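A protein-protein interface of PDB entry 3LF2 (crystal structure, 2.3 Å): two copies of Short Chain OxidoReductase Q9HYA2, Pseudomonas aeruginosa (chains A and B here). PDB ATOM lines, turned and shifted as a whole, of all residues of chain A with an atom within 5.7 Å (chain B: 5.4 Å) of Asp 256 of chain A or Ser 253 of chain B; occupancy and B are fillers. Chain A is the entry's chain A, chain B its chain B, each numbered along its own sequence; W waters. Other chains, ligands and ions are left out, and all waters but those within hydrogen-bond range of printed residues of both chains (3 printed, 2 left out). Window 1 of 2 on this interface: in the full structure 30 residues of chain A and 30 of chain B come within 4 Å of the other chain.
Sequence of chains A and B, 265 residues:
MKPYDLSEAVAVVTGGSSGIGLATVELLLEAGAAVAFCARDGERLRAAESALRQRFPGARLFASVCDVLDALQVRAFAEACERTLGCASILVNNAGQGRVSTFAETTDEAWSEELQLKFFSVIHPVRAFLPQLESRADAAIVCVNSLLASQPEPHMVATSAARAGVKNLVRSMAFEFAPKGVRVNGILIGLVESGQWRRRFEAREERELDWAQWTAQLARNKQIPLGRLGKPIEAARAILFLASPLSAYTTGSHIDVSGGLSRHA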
ATOM      1  N   LEU A 147      17.758  -0.880  -2.201  1.00  0.00           N
ATOM      2  CA  LEU A 147      18.909  -0.680  -3.099  1.00  0.00           C
ATOM      3  C   LEU A 147      20.253  -0.940  -2.384  1.00  0.00           C
ATOM      4  O   LEU A 147      21.262  -1.278  -3.022  1.00  0.00           O
ATOM      5  CB  LEU A 147      18.882   0.725  -3.720  1.00  0.00           C
ATOM      6  CG  LEU A 147      19.883   1.031  -4.850  1.00  0.00           C
ATOM      7  CD1 LEU A 147      19.758   0.018  -5.979  1.00  0.00           C
ATOM      8  CD2 LEU A 147      19.695   2.446  -5.400  1.00  0.00           C
ATOM      9  N   ILE A 187      11.794  -6.407  -4.542  1.00  0.00           N
ATOM     10  CA  ILE A 187      11.982  -5.050  -5.019  1.00  0.00           C
ATOM     11  C   ILE A 187      13.141  -4.462  -4.232  1.00  0.00           C
ATOM     12  O   ILE A 187      13.521  -4.993  -3.183  1.00  0.00           O
ATOM     13  CB  ILE A 187      10.703  -4.185  -4.860  1.00  0.00           C
ATOM     14  CG1 ILE A 187      10.405  -3.923  -3.386  1.00  0.00           C
ATOM     15  CG2 ILE A 187       9.506  -4.857  -5.542  1.00  0.00           C
ATOM     16  CD1 ILE A 187       9.278  -2.931  -3.136  1.00  0.00           C
ATOM     17  N   LEU A 188      13.726  -3.397  -4.767  1.00  0.00           N
ATOM     18  CA  LEU A 188      14.803  -2.678  -4.107  1.00  0.00           C
ATOM     19  C   LEU A 188      14.360  -1.231  -3.962  1.00  0.00           C
ATOM     20  O   LEU A 188      14.451  -0.438  -4.922  1.00  0.00           O
ATOM     21  CB  LEU A 188      16.086  -2.741  -4.941  1.00  0.00           C
ATOM     22  CG  LEU A 188      16.540  -4.147  -5.335  1.00  0.00           C
ATOM     23  CD1 LEU A 188      17.711  -4.090  -6.318  1.00  0.00           C
ATOM     24  CD2 LEU A 188      16.905  -4.938  -4.089  1.00  0.00           C
ATOM     25  N   HIS A 254      14.674  -8.695  -9.506  1.00  0.00           N
ATOM     26  CA  HIS A 254      14.247  -7.591  -8.670  1.00  0.00           C
ATOM     27  C   HIS A 254      13.746  -6.420  -9.521  1.00  0.00           C
ATOM     28  O   HIS A 254      14.191  -6.222 -10.665  1.00  0.00           O
ATOM     29  CB  HIS A 254      15.401  -7.142  -7.769  1.00  0.00           C
ATOM     30  CG  HIS A 254      15.580  -7.995  -6.552  1.00  0.00           C
ATOM     31  ND1 HIS A 254      16.202  -9.225  -6.587  1.00  0.00           N
ATOM     32  CD2 HIS A 254      15.197  -7.805  -5.261  1.00  0.00           C
ATOM     33  CE1 HIS A 254      16.201  -9.749  -5.374  1.00  0.00           C
ATOM     34  NE2 HIS A 254      15.596  -8.908  -4.553  1.00  0.00           N
ATOM     35  N   ILE A 255      12.818  -5.652  -8.954  1.00  0.00           N
ATOM     36  CA  ILE A 255      12.403  -4.392  -9.541  1.00  0.00           C
ATOM     37  C   ILE A 255      12.933  -3.226  -8.713  1.00  0.00           C
ATOM     38  O   ILE A 255      12.791  -3.213  -7.482  1.00  0.00           O
ATOM     39  CB  ILE A 255      10.869  -4.278  -9.665  1.00  0.00           C
ATOM     40  CG1 ILE A 255      10.335  -5.203 -10.778  1.00  0.00           C
ATOM     41  CG2 ILE A 255      10.490  -2.833  -9.929  1.00  0.00           C
ATOM     42  CD1 ILE A 255       8.786  -5.318 -10.799  1.00  0.00           C
ATOM     43  N   ASP A 256      13.533  -2.255  -9.403  1.00  0.00           N
ATOM     44  CA  ASP A 256      14.134  -1.071  -8.792  1.00  0.00           C
ATOM     45  C   ASP A 256      13.060  -0.030  -8.467  1.00  0.00           C
ATOM     46  O   ASP A 256      12.370   0.452  -9.365  1.00  0.00           O
ATOM     47  CB  ASP A 256      15.182  -0.499  -9.761  1.00  0.00           C
ATOM     48  CG  ASP A 256      15.920   0.726  -9.219  1.00  0.00           C
ATOM     49  OD1 ASP A 256      15.360   1.499  -8.415  1.00  0.00           O
ATOM     50  OD2 ASP A 256      17.081   0.934  -9.648  1.00  0.00           O
ATOM     51  N   VAL A 257      12.915   0.313  -7.187  1.00  0.00           N
ATOM     52  CA  VAL A 257      11.941   1.328  -6.761  1.00  0.00           C
ATOM     53  C   VAL A 257      12.655   2.402  -5.935  1.00  0.00           C
ATOM     54  O   VAL A 257      12.299   2.665  -4.774  1.00  0.00           O
ATOM     55  CB  VAL A 257      10.732   0.704  -5.991  1.00  0.00           C
ATOM     56  CG1 VAL A 257       9.674   1.759  -5.653  1.00  0.00           C
ATOM     57  CG2 VAL A 257      10.101  -0.423  -6.797  1.00  0.00           C
ATOM     58  N   SER A 258      13.668   3.010  -6.560  1.00  0.00           N
ATOM     59  CA  SER A 258      14.605   3.915  -5.892  1.00  0.00           C
ATOM     60  C   SER A 258      14.602   5.353  -6.457  1.00  0.00           C
ATOM     61  O   SER A 258      15.293   6.230  -5.938  1.00  0.00           O
ATOM     62  CB  SER A 258      16.024   3.344  -5.997  1.00  0.00           C
ATOM     63  OG  SER A 258      16.524   3.453  -7.325  1.00  0.00           O
ATOM     64  N   GLY A 259      13.839   5.593  -7.519  1.00  0.00           N
ATOM     65  CA  GLY A 259      13.772   6.923  -8.109  1.00  0.00           C
ATOM     66  C   GLY A 259      15.041   7.281  -8.871  1.00  0.00           C
ATOM     67  O   GLY A 259      15.430   8.439  -8.945  1.00  0.00           O
ATOM     68  N   GLY A 260      15.690   6.276  -9.442  1.00  0.00           N
ATOM     69  CA  GLY A 260      16.928   6.477 -10.173  1.00  0.00           C
ATOM     70  C   GLY A 260      18.225   6.576  -9.365  1.00  0.00           C
ATOM     71  O   GLY A 260      19.174   7.202  -9.814  1.00  0.00           O
ATOM     72  N   LEU A 261      18.288   5.940  -8.196  1.00  0.00           N
ATOM     73  CA  LEU A 261      19.500   6.027  -7.363  1.00  0.00           C
ATOM     74  C   LEU A 261      20.614   5.030  -7.730  1.00  0.00           C
ATOM     75  O   LEU A 261      21.755   5.176  -7.295  1.00  0.00           O
ATOM     76  CB  LEU A 261      19.146   5.871  -5.878  1.00  0.00           C
ATOM     77  CG  LEU A 261      18.788   7.121  -5.074  1.00  0.00           C
ATOM     78  CD1 LEU A 261      18.465   6.724  -3.648  1.00  0.00           C
ATOM     79  CD2 LEU A 261      19.931   8.141  -5.105  1.00  0.00           C
ATOM     80  N   SER A 262      20.279   4.013  -8.516  1.00  0.00           N
ATOM     81  CA  SER A 262      21.247   2.969  -8.853  1.00  0.00           C
ATOM     82  C   SER A 262      22.228   3.433  -9.923  1.00  0.00           C
ATOM     83  O   SER A 262      21.849   3.639 -11.094  1.00  0.00           O
ATOM     84  CB  SER A 262      20.555   1.684  -9.304  1.00  0.00           C
ATOM     85  OG  SER A 262      21.516   0.706  -9.668  1.00  0.00           O
ATOM     86  N   VAL B 170      20.522   3.223 -21.605  1.00  0.00           N
ATOM     87  CA  VAL B 170      19.274   3.420 -20.890  1.00  0.00           C
ATOM     88  C   VAL B 170      19.509   4.066 -19.533  1.00  0.00           C
ATOM     89  O   VAL B 170      18.795   4.992 -19.158  1.00  0.00           O
ATOM     90  CB  VAL B 170      18.479   2.129 -20.747  1.00  0.00           C
ATOM     91  CG1 VAL B 170      17.372   2.312 -19.714  1.00  0.00           C
ATOM     92  CG2 VAL B 170      17.896   1.730 -22.107  1.00  0.00           C
ATOM     93  N   VAL B 184      13.020   6.436 -17.897  1.00  0.00           N
ATOM     94  CA  VAL B 184      13.572   5.584 -18.942  1.00  0.00           C
ATOM     95  C   VAL B 184      13.983   4.233 -18.377  1.00  0.00           C
ATOM     96  O   VAL B 184      14.851   4.165 -17.525  1.00  0.00           O
ATOM     97  CB  VAL B 184      14.841   6.200 -19.581  1.00  0.00           C
ATOM     98  CG1 VAL B 184      15.333   5.314 -20.701  1.00  0.00           C
ATOM     99  CG2 VAL B 184      14.577   7.609 -20.072  1.00  0.00           C
ATOM    100  N   ASN B 185      13.387   3.159 -18.878  1.00  0.00           N
ATOM    101  CA  ASN B 185      13.707   1.824 -18.405  1.00  0.00           C
ATOM    102  C   ASN B 185      13.859   0.858 -19.572  1.00  0.00           C
ATOM    103  O   ASN B 185      13.679   1.242 -20.714  1.00  0.00           O
ATOM    104  CB  ASN B 185      12.634   1.337 -17.421  1.00  0.00           C
ATOM    105  CG  ASN B 185      12.519   2.230 -16.187  1.00  0.00           C
ATOM    106  OD1 ASN B 185      13.348   2.165 -15.272  1.00  0.00           O
ATOM    107  ND2 ASN B 185      11.488   3.067 -16.157  1.00  0.00           N
ATOM    108  N   GLY B 186      14.206  -0.393 -19.283  1.00  0.00           N
ATOM    109  CA  GLY B 186      14.149  -1.440 -20.289  1.00  0.00           C
ATOM    110  C   GLY B 186      13.607  -2.748 -19.728  1.00  0.00           C
ATOM    111  O   GLY B 186      13.387  -2.888 -18.523  1.00  0.00           O
ATOM    112  N   LEU B 242       6.205  -0.566 -16.892  1.00  0.00           N
ATOM    113  CA  LEU B 242       7.251   0.465 -16.950  1.00  0.00           C
ATOM    114  C   LEU B 242       6.808   1.761 -17.671  1.00  0.00           C
ATOM    115  O   LEU B 242       7.293   2.856 -17.360  1.00  0.00           O
ATOM    116  CB  LEU B 242       8.546  -0.097 -17.588  1.00  0.00           C
ATOM    117  CG  LEU B 242       9.357  -1.146 -16.787  1.00  0.00           C
ATOM    118  CD1 LEU B 242      10.597  -1.656 -17.539  1.00  0.00           C
ATOM    119  CD2 LEU B 242       9.761  -0.621 -15.403  1.00  0.00           C
ATOM    120  N   TYR B 249       8.036   5.623  -9.666  1.00  0.00           N
ATOM    121  CA  TYR B 249       9.277   5.863  -8.924  1.00  0.00           C
ATOM    122  C   TYR B 249      10.399   4.921  -9.385  1.00  0.00           C
ATOM    123  O   TYR B 249      11.310   4.583  -8.622  1.00  0.00           O
ATOM    124  CB  TYR B 249       9.017   5.706  -7.426  1.00  0.00           C
ATOM    125  CG  TYR B 249       9.981   6.456  -6.540  1.00  0.00           C
ATOM    126  CD1 TYR B 249      10.003   7.845  -6.528  1.00  0.00           C
ATOM    127  CD2 TYR B 249      10.863   5.777  -5.702  1.00  0.00           C
ATOM    128  CE1 TYR B 249      10.887   8.541  -5.715  1.00  0.00           C
ATOM    129  CE2 TYR B 249      11.748   6.465  -4.879  1.00  0.00           C
ATOM    130  CZ  TYR B 249      11.752   7.849  -4.889  1.00  0.00           C
ATOM    131  OH  TYR B 249      12.621   8.546  -4.077  1.00  0.00           O
ATOM    132  N   THR B 250      10.320   4.509 -10.649  1.00  0.00           N
ATOM    133  CA  THR B 250      11.277   3.581 -11.243  1.00  0.00           C
ATOM    134  C   THR B 250      11.897   4.202 -12.482  1.00  0.00           C
ATOM    135  O   THR B 250      11.235   4.374 -13.494  1.00  0.00           O
ATOM    136  CB  THR B 250      10.584   2.273 -11.664  1.00  0.00           C
ATOM    137  OG1 THR B 250      10.103   1.591 -10.498  1.00  0.00           O
ATOM    138  CG2 THR B 250      11.542   1.370 -12.439  1.00  0.00           C
ATOM    139  N   THR B 251      13.169   4.561 -12.413  1.00  0.00           N
ATOM    140  CA  THR B 251      13.837   5.026 -13.613  1.00  0.00           C
ATOM    141  C   THR B 251      15.278   4.544 -13.661  1.00  0.00           C
ATOM    142  O   THR B 251      15.924   4.380 -12.620  1.00  0.00           O
ATOM    143  CB  THR B 251      13.760   6.552 -13.763  1.00  0.00           C
ATOM    144  OG1 THR B 251      14.161   6.927 -15.093  1.00  0.00           O
ATOM    145  CG2 THR B 251      14.623   7.242 -12.725  1.00  0.00           C
ATOM    146  N   GLY B 252      15.761   4.299 -14.876  1.00  0.00           N
ATOM    147  CA  GLY B 252      17.128   3.860 -15.089  1.00  0.00           C
ATOM    148  C   GLY B 252      17.321   2.408 -14.721  1.00  0.00           C
ATOM    149  O   GLY B 252      18.383   2.025 -14.249  1.00  0.00           O
ATOM    150  N   SER B 253      16.294   1.591 -14.923  1.00  0.00           N
ATOM    151  CA  SER B 253      16.357   0.202 -14.473  1.00  0.00           C
ATOM    152  C   SER B 253      15.852  -0.744 -15.541  1.00  0.00           C
ATOM    153  O   SER B 253      15.485  -0.321 -16.635  1.00  0.00           O
ATOM    154  CB  SER B 253      15.515   0.002 -13.211  1.00  0.00           C
ATOM    155  OG  SER B 253      14.149  -0.182 -13.554  1.00  0.00           O
ATOM    156  N   HIS B 254      15.812  -2.026 -15.208  1.00  0.00           N
ATOM    157  CA  HIS B 254      15.314  -3.025 -16.134  1.00  0.00           C
ATOM    158  C   HIS B 254      14.470  -4.074 -15.432  1.00  0.00           C
ATOM    159  O   HIS B 254      14.677  -4.382 -14.249  1.00  0.00           O
ATOM    160  CB  HIS B 254      16.483  -3.695 -16.866  1.00  0.00           C
ATOM    161  CG  HIS B 254      17.053  -2.868 -17.982  1.00  0.00           C
ATOM    162  ND1 HIS B 254      17.901  -1.803 -17.763  1.00  0.00           N
ATOM    163  CD2 HIS B 254      16.900  -2.956 -19.325  1.00  0.00           C
ATOM    164  CE1 HIS B 254      18.237  -1.266 -18.921  1.00  0.00           C
ATOM    165  NE2 HIS B 254      17.643  -1.946 -19.885  1.00  0.00           N
ATOM    166  N   ILE B 255      13.509  -4.623 -16.165  1.00  0.00           N
ATOM    167  CA  ILE B 255      12.777  -5.778 -15.674  1.00  0.00           C
ATOM    168  C   ILE B 255      13.175  -7.022 -16.458  1.00  0.00           C
ATOM    169  O   ILE B 255      13.239  -7.015 -17.696  1.00  0.00           O
ATOM    170  CB  ILE B 255      11.252  -5.568 -15.720  1.00  0.00           C
ATOM    171  CG1 ILE B 255      10.821  -4.481 -14.732  1.00  0.00           C
ATOM    172  CG2 ILE B 255      10.527  -6.864 -15.414  1.00  0.00           C
ATOM    173  CD1 ILE B 255       9.334  -4.112 -14.842  1.00  0.00           C
HETATM  174  O   HOH W   1      14.881   7.181  -3.361  1.00  0.00           O
HETATM  175  O   HOH W   2      17.977   3.535  -9.995  1.00  0.00           O
HETATM  176  O   HOH W   3      13.586  -2.675 -12.473  1.00  0.00           O
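Asp 256 of chain A touches Ser 253 of chain B (CB to CB, 3.5 Å). Tyr 249 of chain B touches Val 257 of chain A. Tyr 249 of chain B touches Ser 258 of chain A (CE2 to C, 3.4 Å). Gly 259 of chain A touches Thr 251 of chain B (C to CG2, 3.9 Å). CA of Gly 260 of chain A touches O of Thr 251 of chain B, 3.4 Å away.
Positions printed for both chains: 254 and 255.
Water W3 lies within hydrogen-bond range of the backbone carbonyl oxygen of His 254 of chain B (2.7 Å), the side-chain hydroxyl of Ser 253 of chain B (2.8 Å) and the backbone NH of Asp 256 of chain A (3.1 Å). Water W1 lies within hydrogen-bond range of OH of Tyr 249 of chain B (2.7 Å) and O of Ser 258 of chain A (2.8 Å). Water W2 lies within hydrogen-bond range of OD2 of Asp 256 of chain A (2.8 Å), N of Ser 262 of chain A (2.8 Å), N of Leu 261 of chain A (3.0 Å), OG of Ser 258 of chain A (3.0 Å) and O of Thr 251 of chain B (3.4 Å).
The backbone carbonyl oxygen (O) of Leu 188 of chain A is in hydrogen-bond range of the backbone NH (N) of Val 257 of chain A (2.8 Å). OD1 of Asp 256 of chain A lies within hydrogen-bond range of OG of Ser 258 of chain A (2.5 Å). OG of Ser 258 of chain A sits at hydrogen-bond distance from N of Leu 261 of chain A (3.2 Å). O of Thr 250 of chain B is in hydrogen-bond range of ND2 of Asn 185 of chain B, at 3.0 Å. The side-chain amide oxygen (OD1) of Asn 185 of chain B sits at hydrogen-bond distance from the side-chain hydroxyl (OG) of Ser 253 of chain B, at 3.0 Å. N of Gly 186 of chain B sits at hydrogen-bond distance from O of Ser 253 of chain B, at 2.9 Å.
The side-chain hydroxyl (OG1) of Thr 250 of chain B sits at hydrogen-bond distance from the backbone carbonyl oxygen (O) of Asp 256 of chain A (2.8 Å). The backbone carbonyl oxygen (O) of Tyr 249 of chain B sits at hydrogen-bond distance from the backbone NH (N) of Gly 259 of chain A, 2.9 Å away.
Asp 256 of chain A touches just these residues of chain B: Thr 250 (2.8 Å) and Ser 253 (3.5 Å). Of the printed residues of chain B, Ser 258 of chain A touches Tyr 249 (3.4 Å). Of the printed residues of chain B, Gly 260 of chain A touches Thr 251 (3.4 Å). Printed residues of chain A within 4 Å of Tyr 249 of chain B: Val 257 (3.6 Å), Ser 258 (3.4 Å) and Gly 259 (2.9 Å). Of the printed residues of chain A, Thr 250 of chain B touches Asp 256. Ser 253 of chain B touches one residue of chain A. The nearest residue of chain B that does not touch Asp 256 of chain A is Tyr 249 of chain B (4.3 Å).
Of the 12 printed residues of chain A, 5 touch a printed residue of chain B. Printed residues of chain B that touch a printed residue of chain A: Tyr 249, Thr 250, Thr 251 and Ser 253. Hydrophobic or aromatic side chains of chain B within 4 Å of the printed part of chain A: Tyr 249.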
